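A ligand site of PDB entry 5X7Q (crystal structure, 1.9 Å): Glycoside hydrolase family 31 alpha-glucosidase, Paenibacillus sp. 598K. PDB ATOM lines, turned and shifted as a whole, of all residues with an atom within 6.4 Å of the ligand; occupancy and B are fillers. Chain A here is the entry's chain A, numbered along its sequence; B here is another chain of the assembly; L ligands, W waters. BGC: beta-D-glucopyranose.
OD2 of Asp 293 of chain B lies within hydrogen-bond range of O4 of the ligand (2.6 Å).
OD2 of Asp 411 sits at hydrogen-bond distance from O1 of the ligand (2.6 Å).
The side-chain carboxylate (OD1) of Asp 473 lies within hydrogen-bond range of an oxygen (O2) of the ligand, at 2.7 Å.
NZ of Lys 338 of chain B is in hydrogen-bond range of O6 of the ligand (2.7 Å).
NE2 of His 547 lies within hydrogen-bond range of O4 of the ligand (2.8 Å).
The guanidinium group (NH1) of Arg 456 lies within hydrogen-bond range of an oxygen (O1) of the ligand (2.9 Å).
An oxygen (O1) of the ligand lies within hydrogen-bond range of the side-chain carboxylate (OE2) of Glu 412 (3.2 Å).
OD2 of Asp 411 lies within salt-bridge range of NZ of Lys 338 of chain B (2.8 Å).
The side-chain carboxylate (OD1) of Asp 411 lies within salt-bridge range of the guanidinium group (NH1) of Arg 456 (3.2 Å).
The backbone NH (N) of Asp 473 lies within hydrogen-bond range of the side-chain amide oxygen (OE1) of Gln 176 of chain B, 3.0 Å away.
NZ of Lys 338 of chain B lies within salt-bridge range of OE1 of Glu 412.
The side-chain carboxylate of Asp 511 sits close to the indole nitrogen of Trp 470, 3.5 Å away.
Residues that only touch the ligand: Tyr 294 of chain B (3.4 Å), Ile 336 of chain B (3.4 Å), Phe 515 (3.4 Å), Trp 409 (3.4 Å), Trp 266 of chain B (3.5 Å) and Trp 470 (3.7 Å).
Hydrophobic or aromatic side chains within 4 Å of the ligand: Trp 409, Trp 470, Phe 515, His 547, Trp 266 of chain B, Tyr 294 of chain B and Ile 336 of chain B.
Of the 21 residues printed, 13 come within 4 Å of the ligand.
Water W1 lies within hydrogen-bond range of OE2 of Glu 412, O5 of the ligand and NZ of Lys 338 of chain B.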
ATOM      1  N   TRP A 409     -16.529   5.726  20.628  1.00  0.00           N
ATOM      2  CA  TRP A 409     -15.617   4.620  20.418  1.00  0.00           C
ATOM      3  C   TRP A 409     -14.282   5.236  20.023  1.00  0.00           C
ATOM      4  O   TRP A 409     -14.035   5.524  18.866  1.00  0.00           O
ATOM      5  CB  TRP A 409     -16.237   3.689  19.383  1.00  0.00           C
ATOM      6  CG  TRP A 409     -15.425   2.626  18.806  1.00  0.00           C
ATOM      7  CD1 TRP A 409     -14.258   2.112  19.271  1.00  0.00           C
ATOM      8  CD2 TRP A 409     -15.749   1.903  17.622  1.00  0.00           C
ATOM      9  NE1 TRP A 409     -13.823   1.107  18.431  1.00  0.00           N
ATOM     10  CE2 TRP A 409     -14.721   0.953  17.410  1.00  0.00           C
ATOM     11  CE3 TRP A 409     -16.826   1.950  16.717  1.00  0.00           C
ATOM     12  CZ2 TRP A 409     -14.722   0.080  16.321  1.00  0.00           C
ATOM     13  CZ3 TRP A 409     -16.823   1.082  15.636  1.00  0.00           C
ATOM     14  CH2 TRP A 409     -15.771   0.164  15.445  1.00  0.00           C
ATOM     15  N   ASP A 411     -10.793   5.289  19.185  1.00  0.00           N
ATOM     16  CA  ASP A 411      -9.773   4.376  18.661  1.00  0.00           C
ATOM     17  C   ASP A 411      -8.429   5.082  18.526  1.00  0.00           C
ATOM     18  O   ASP A 411      -8.366   6.309  18.451  1.00  0.00           O
ATOM     19  CB  ASP A 411     -10.234   3.830  17.312  1.00  0.00           C
ATOM     20  CG  ASP A 411      -9.278   2.805  16.732  1.00  0.00           C
ATOM     21  OD1 ASP A 411      -8.697   2.020  17.503  1.00  0.00           O
ATOM     22  OD2 ASP A 411      -9.104   2.786  15.493  1.00  0.00           O
ATOM     23  N   GLU A 412      -7.350   4.296  18.552  1.00  0.00           N
ATOM     24  CA  GLU A 412      -6.021   4.768  18.147  1.00  0.00           C
ATOM     25  C   GLU A 412      -5.537   5.973  18.970  1.00  0.00           C
ATOM     26  O   GLU A 412      -4.906   6.897  18.441  1.00  0.00           O
ATOM     27  CB  GLU A 412      -5.984   5.053  16.618  1.00  0.00           C
ATOM     28  CG  GLU A 412      -5.762   3.787  15.804  1.00  0.00           C
ATOM     29  CD  GLU A 412      -5.969   3.926  14.292  1.00  0.00           C
ATOM     30  OE1 GLU A 412      -6.538   4.933  13.811  1.00  0.00           O
ATOM     31  OE2 GLU A 412      -5.590   2.988  13.566  1.00  0.00           O
ATOM     32  N   ARG A 456      -8.778   1.539  23.458  1.00  0.00           N
ATOM     33  CA  ARG A 456      -7.979   0.309  23.413  1.00  0.00           C
ATOM     34  C   ARG A 456      -6.664   0.406  24.168  1.00  0.00           C
ATOM     35  O   ARG A 456      -5.722  -0.321  23.891  1.00  0.00           O
ATOM     36  CB  ARG A 456      -7.793  -0.185  21.978  1.00  0.00           C
ATOM     37  CG  ARG A 456      -6.957   0.674  21.107  1.00  0.00           C
ATOM     38  CD  ARG A 456      -6.910   0.093  19.702  1.00  0.00           C
ATOM     39  NE  ARG A 456      -5.750   0.643  19.031  1.00  0.00           N
ATOM     40  CZ  ARG A 456      -5.503   0.587  17.727  1.00  0.00           C
ATOM     41  NH1 ARG A 456      -6.338   0.008  16.865  1.00  0.00           N
ATOM     42  NH2 ARG A 456      -4.373   1.133  17.289  1.00  0.00           N
ATOM     43  N   TRP A 470     -11.362  -2.126  25.311  1.00  0.00           N
ATOM     44  CA  TRP A 470     -11.499  -3.329  24.457  1.00  0.00           C
ATOM     45  C   TRP A 470     -10.110  -3.816  24.030  1.00  0.00           C
ATOM     46  O   TRP A 470      -9.167  -3.023  23.991  1.00  0.00           O
ATOM     47  CB  TRP A 470     -12.458  -3.111  23.297  1.00  0.00           C
ATOM     48  CG  TRP A 470     -11.890  -2.747  21.941  1.00  0.00           C
ATOM     49  CD1 TRP A 470     -11.617  -3.606  20.913  1.00  0.00           C
ATOM     50  CD2 TRP A 470     -11.634  -1.433  21.449  1.00  0.00           C
ATOM     51  NE1 TRP A 470     -11.146  -2.917  19.849  1.00  0.00           N
ATOM     52  CE2 TRP A 470     -11.154  -1.581  20.127  1.00  0.00           C
ATOM     53  CE3 TRP A 470     -11.745  -0.142  21.999  1.00  0.00           C
ATOM     54  CZ2 TRP A 470     -10.761  -0.487  19.350  1.00  0.00           C
ATOM     55  CZ3 TRP A 470     -11.355   0.947  21.214  1.00  0.00           C
ATOM     56  CH2 TRP A 470     -10.862   0.769  19.893  1.00  0.00           C
ATOM     57  N   GLY A 472      -8.548  -4.746  21.349  1.00  0.00           N
ATOM     58  CA  GLY A 472      -7.918  -4.384  20.093  1.00  0.00           C
ATOM     59  C   GLY A 472      -8.152  -5.384  18.981  1.00  0.00           C
ATOM     60  O   GLY A 472      -9.079  -6.185  19.045  1.00  0.00           O
ATOM     61  N   ASP A 473      -7.281  -5.368  17.979  1.00  0.00           N
ATOM     62  CA  ASP A 473      -7.481  -6.104  16.721  1.00  0.00           C
ATOM     63  C   ASP A 473      -7.074  -7.585  16.837  1.00  0.00           C
ATOM     64  O   ASP A 473      -6.175  -8.066  16.135  1.00  0.00           O
ATOM     65  CB  ASP A 473      -6.718  -5.438  15.577  1.00  0.00           C
ATOM     66  CG  ASP A 473      -7.214  -4.037  15.249  1.00  0.00           C
ATOM     67  OD1 ASP A 473      -8.315  -3.621  15.685  1.00  0.00           O
ATOM     68  OD2 ASP A 473      -6.490  -3.351  14.510  1.00  0.00           O
ATOM     69  N   ASP A 511     -13.446  -7.992  20.720  1.00  0.00           N
ATOM     70  CA  ASP A 511     -14.117  -8.185  19.444  1.00  0.00           C
ATOM     71  C   ASP A 511     -14.545  -9.649  19.367  1.00  0.00           C
ATOM     72  O   ASP A 511     -13.753 -10.511  18.933  1.00  0.00           O
ATOM     73  CB  ASP A 511     -13.185  -7.899  18.244  1.00  0.00           C
ATOM     74  CG  ASP A 511     -12.759  -6.444  18.132  1.00  0.00           C
ATOM     75  OD1 ASP A 511     -13.224  -5.551  18.880  1.00  0.00           O
ATOM     76  OD2 ASP A 511     -11.909  -6.190  17.239  1.00  0.00           O
ATOM     77  N   PHE A 515     -11.184  -9.863  14.860  1.00  0.00           N
ATOM     78  CA  PHE A 515     -11.004  -8.818  13.874  1.00  0.00           C
ATOM     79  C   PHE A 515     -10.103  -9.249  12.725  1.00  0.00           C
ATOM     80  O   PHE A 515     -10.446  -9.024  11.579  1.00  0.00           O
ATOM     81  CB  PHE A 515     -10.424  -7.583  14.545  1.00  0.00           C
ATOM     82  CG  PHE A 515     -10.369  -6.375  13.641  1.00  0.00           C
ATOM     83  CD1 PHE A 515     -11.463  -5.517  13.529  1.00  0.00           C
ATOM     84  CD2 PHE A 515      -9.214  -6.099  12.905  1.00  0.00           C
ATOM     85  CE1 PHE A 515     -11.406  -4.414  12.699  1.00  0.00           C
ATOM     86  CE2 PHE A 515      -9.157  -4.996  12.075  1.00  0.00           C
ATOM     87  CZ  PHE A 515     -10.255  -4.139  11.976  1.00  0.00           C
ATOM     88  N   ARG A 545     -19.925  -7.394  23.036  1.00  0.00           N
ATOM     89  CA  ARG A 545     -19.938  -6.798  21.693  1.00  0.00           C
ATOM     90  C   ARG A 545     -19.274  -7.678  20.656  1.00  0.00           C
ATOM     91  O   ARG A 545     -18.239  -8.269  20.936  1.00  0.00           O
ATOM     92  CB  ARG A 545     -19.253  -5.437  21.713  1.00  0.00           C
ATOM     93  CG  ARG A 545     -17.812  -5.471  22.243  1.00  0.00           C
ATOM     94  CD  ARG A 545     -17.182  -4.085  22.317  1.00  0.00           C
ATOM     95  NE  ARG A 545     -16.642  -3.598  21.055  1.00  0.00           N
ATOM     96  CZ  ARG A 545     -15.533  -4.051  20.467  1.00  0.00           C
ATOM     97  NH1 ARG A 545     -14.845  -5.071  20.973  1.00  0.00           N
ATOM     98  NH2 ARG A 545     -15.113  -3.508  19.326  1.00  0.00           N
ATOM     99  N   HIS A 547     -17.534  -7.577  16.777  1.00  0.00           N
ATOM    100  CA  HIS A 547     -16.898  -6.673  15.805  1.00  0.00           C
ATOM    101  C   HIS A 547     -16.168  -7.538  14.784  1.00  0.00           C
ATOM    102  O   HIS A 547     -15.933  -8.737  15.013  1.00  0.00           O
ATOM    103  CB  HIS A 547     -15.957  -5.680  16.501  1.00  0.00           C
ATOM    104  CG  HIS A 547     -15.424  -4.590  15.603  1.00  0.00           C
ATOM    105  ND1 HIS A 547     -16.170  -4.016  14.603  1.00  0.00           N
ATOM    106  CD2 HIS A 547     -14.228  -3.961  15.605  1.00  0.00           C
ATOM    107  CE1 HIS A 547     -15.442  -3.107  13.986  1.00  0.00           C
ATOM    108  NE2 HIS A 547     -14.261  -3.038  14.586  1.00  0.00           N
ATOM    109  N   GLY A 548     -15.908  -6.966  13.624  1.00  0.00           N
ATOM    110  CA  GLY A 548     -15.131  -7.631  12.587  1.00  0.00           C
ATOM    111  C   GLY A 548     -14.483  -6.590  11.712  1.00  0.00           C
ATOM    112  O   GLY A 548     -14.746  -5.381  11.854  1.00  0.00           O
ATOM    113  N   ASN A 549     -13.664  -7.069  10.782  1.00  0.00           N
ATOM    114  CA  ASN A 549     -12.936  -6.218   9.857  1.00  0.00           C
ATOM    115  C   ASN A 549     -13.890  -5.647   8.789  1.00  0.00           C
ATOM    116  O   ASN A 549     -15.094  -5.909   8.789  1.00  0.00           O
ATOM    117  CB  ASN A 549     -11.797  -7.024   9.213  1.00  0.00           C
ATOM    118  CG  ASN A 549     -10.593  -6.183   8.864  1.00  0.00           C
ATOM    119  OD1 ASN A 549     -10.726  -5.024   8.474  1.00  0.00           O
ATOM    120  ND2 ASN A 549      -9.407  -6.780   8.946  1.00  0.00           N
ATOM    121  N   TYR A 550     -13.330  -4.840   7.903  1.00  0.00           N
ATOM    122  CA  TYR A 550     -14.096  -4.095   6.893  1.00  0.00           C
ATOM    123  C   TYR A 550     -15.001  -4.996   6.079  1.00  0.00           C
ATOM    124  O   TYR A 550     -14.530  -5.984   5.509  1.00  0.00           O
ATOM    125  CB  TYR A 550     -13.148  -3.369   5.938  1.00  0.00           C
ATOM    126  CG  TYR A 550     -13.868  -2.553   4.870  1.00  0.00           C
ATOM    127  CD1 TYR A 550     -14.694  -1.489   5.220  1.00  0.00           C
ATOM    128  CD2 TYR A 550     -13.710  -2.852   3.511  1.00  0.00           C
ATOM    129  CE1 TYR A 550     -15.333  -0.730   4.253  1.00  0.00           C
ATOM    130  CE2 TYR A 550     -14.343  -2.088   2.539  1.00  0.00           C
ATOM    131  CZ  TYR A 550     -15.154  -1.033   2.914  1.00  0.00           C
ATOM    132  OH  TYR A 550     -15.771  -0.294   1.951  1.00  0.00           O
ATOM    133  N   GLN B 176      -3.128  -1.238  21.360  1.00  0.00           N
ATOM    134  CA  GLN B 176      -3.804  -2.421  20.815  1.00  0.00           C
ATOM    135  C   GLN B 176      -4.339  -3.352  21.924  1.00  0.00           C
ATOM    136  O   GLN B 176      -4.143  -4.568  21.897  1.00  0.00           O
ATOM    137  CB  GLN B 176      -2.866  -3.153  19.833  1.00  0.00           C
ATOM    138  CG  GLN B 176      -2.836  -2.518  18.450  1.00  0.00           C
ATOM    139  CD  GLN B 176      -4.033  -2.922  17.604  1.00  0.00           C
ATOM    140  OE1 GLN B 176      -5.103  -3.312  18.121  1.00  0.00           O
ATOM    141  NE2 GLN B 176      -3.859  -2.848  16.297  1.00  0.00           N
ATOM    142  N   PHE B 264     -20.856  -3.943  16.783  1.00  0.00           N
ATOM    143  CA  PHE B 264     -19.935  -2.989  16.153  1.00  0.00           C
ATOM    144  C   PHE B 264     -19.775  -3.422  14.716  1.00  0.00           C
ATOM    145  O   PHE B 264     -19.764  -4.610  14.410  1.00  0.00           O
ATOM    146  CB  PHE B 264     -18.551  -2.964  16.840  1.00  0.00           C
ATOM    147  CG  PHE B 264     -18.525  -2.215  18.154  1.00  0.00           C
ATOM    148  CD1 PHE B 264     -19.456  -2.480  19.144  1.00  0.00           C
ATOM    149  CD2 PHE B 264     -17.549  -1.243  18.386  1.00  0.00           C
ATOM    150  CE1 PHE B 264     -19.441  -1.779  20.345  1.00  0.00           C
ATOM    151  CE2 PHE B 264     -17.519  -0.555  19.589  1.00  0.00           C
ATOM    152  CZ  PHE B 264     -18.460  -0.818  20.569  1.00  0.00           C
ATOM    153  N   TRP B 266     -18.042  -2.178  10.654  1.00  0.00           N
ATOM    154  CA  TRP B 266     -17.358  -1.359   9.667  1.00  0.00           C
ATOM    155  C   TRP B 266     -17.838  -1.879   8.321  1.00  0.00           C
ATOM    156  O   TRP B 266     -17.717  -3.063   8.033  1.00  0.00           O
ATOM    157  CB  TRP B 266     -15.850  -1.519   9.857  1.00  0.00           C
ATOM    158  CG  TRP B 266     -14.951  -0.683   8.976  1.00  0.00           C
ATOM    159  CD1 TRP B 266     -15.301   0.404   8.207  1.00  0.00           C
ATOM    160  CD2 TRP B 266     -13.548  -0.852   8.794  1.00  0.00           C
ATOM    161  NE1 TRP B 266     -14.198   0.894   7.557  1.00  0.00           N
ATOM    162  CE2 TRP B 266     -13.111   0.148   7.899  1.00  0.00           C
ATOM    163  CE3 TRP B 266     -12.614  -1.764   9.303  1.00  0.00           C
ATOM    164  CZ2 TRP B 266     -11.774   0.252   7.491  1.00  0.00           C
ATOM    165  CZ3 TRP B 266     -11.284  -1.649   8.916  1.00  0.00           C
ATOM    166  CH2 TRP B 266     -10.880  -0.656   8.013  1.00  0.00           C
ATOM    167  N   ASP B 293     -18.500   2.463  12.403  1.00  0.00           N
ATOM    168  CA  ASP B 293     -17.099   2.751  12.106  1.00  0.00           C
ATOM    169  C   ASP B 293     -17.029   4.021  11.209  1.00  0.00           C
ATOM    170  O   ASP B 293     -17.928   4.858  11.269  1.00  0.00           O
ATOM    171  CB  ASP B 293     -16.448   1.507  11.440  1.00  0.00           C
ATOM    172  CG  ASP B 293     -14.937   1.398  11.720  1.00  0.00           C
ATOM    173  OD1 ASP B 293     -14.205   2.392  11.442  1.00  0.00           O
ATOM    174  OD2 ASP B 293     -14.492   0.312  12.184  1.00  0.00           O
ATOM    175  N   TYR B 294     -15.958   4.181  10.426  1.00  0.00           N
ATOM    176  CA  TYR B 294     -15.775   5.318   9.517  1.00  0.00           C
ATOM    177  C   TYR B 294     -17.054   5.729   8.774  1.00  0.00           C
ATOM    178  O   TYR B 294     -17.281   6.917   8.524  1.00  0.00           O
ATOM    179  CB  TYR B 294     -14.725   4.994   8.457  1.00  0.00           C
ATOM    180  CG  TYR B 294     -13.286   5.107   8.900  1.00  0.00           C
ATOM    181  CD1 TYR B 294     -12.710   6.345   9.143  1.00  0.00           C
ATOM    182  CD2 TYR B 294     -12.480   3.975   9.014  1.00  0.00           C
ATOM    183  CE1 TYR B 294     -11.386   6.469   9.525  1.00  0.00           C
ATOM    184  CE2 TYR B 294     -11.139   4.086   9.384  1.00  0.00           C
ATOM    185  CZ  TYR B 294     -10.601   5.341   9.619  1.00  0.00           C
ATOM    186  OH  TYR B 294      -9.288   5.499  10.007  1.00  0.00           O
ATOM    187  N   ILE B 336     -17.315   5.781  15.944  1.00  0.00           N
ATOM    188  CA  ILE B 336     -15.853   5.711  16.085  1.00  0.00           C
ATOM    189  C   ILE B 336     -15.249   7.119  15.959  1.00  0.00           C
ATOM    190  O   ILE B 336     -15.711   7.945  15.180  1.00  0.00           O
ATOM    191  CB  ILE B 336     -15.206   4.730  15.090  1.00  0.00           C
ATOM    192  CG1 ILE B 336     -13.829   4.279  15.613  1.00  0.00           C
ATOM    193  CG2 ILE B 336     -15.116   5.321  13.675  1.00  0.00           C
ATOM    194  CD1 ILE B 336     -13.248   3.119  14.848  1.00  0.00           C
ATOM    195  N   LYS B 338     -11.285   9.101  15.929  1.00  0.00           N
ATOM    196  CA  LYS B 338      -9.838   9.006  15.797  1.00  0.00           C
ATOM    197  C   LYS B 338      -9.266  10.328  16.334  1.00  0.00           C
ATOM    198  O   LYS B 338      -9.791  11.395  15.996  1.00  0.00           O
ATOM    199  CB  LYS B 338      -9.464   8.816  14.318  1.00  0.00           C
ATOM    200  CG  LYS B 338     -10.276   7.735  13.602  1.00  0.00           C
ATOM    201  CD  LYS B 338      -9.793   6.335  13.935  1.00  0.00           C
ATOM    202  CE  LYS B 338     -10.668   5.307  13.222  1.00  0.00           C
ATOM    203  NZ  LYS B 338     -10.051   3.950  13.174  1.00  0.00           N
HETATM  204  C2  BGC L   1      -9.717  -0.441  15.197  1.00  0.00           C
HETATM  205  C3  BGC L   1     -10.881  -1.269  14.691  1.00  0.00           C
HETATM  206  C4  BGC L   1     -11.606  -0.476  13.613  1.00  0.00           C
HETATM  207  C5  BGC L   1     -10.636  -0.042  12.495  1.00  0.00           C
HETATM  208  C6  BGC L   1     -11.301   0.836  11.442  1.00  0.00           C
HETATM  209  C1  BGC L   1      -8.799  -0.062  14.021  1.00  0.00           C
HETATM  210  O1  BGC L   1      -7.737   0.776  14.460  1.00  0.00           O
HETATM  211  O2  BGC L   1      -8.966  -1.094  16.230  1.00  0.00           O
HETATM  212  O3  BGC L   1     -11.770  -1.574  15.776  1.00  0.00           O
HETATM  213  O4  BGC L   1     -12.661  -1.270  13.047  1.00  0.00           O
HETATM  214  O5  BGC L   1      -9.548   0.684  13.066  1.00  0.00           O
HETATM  215  O6  BGC L   1     -11.689   2.083  12.023  1.00  0.00           O
HETATM  216  O   HOH W   1      -7.625   2.662  11.783  1.00  0.00           O
HETATM  217  O   HOH W   2     -10.708  -3.831  17.143  1.00  0.00           O
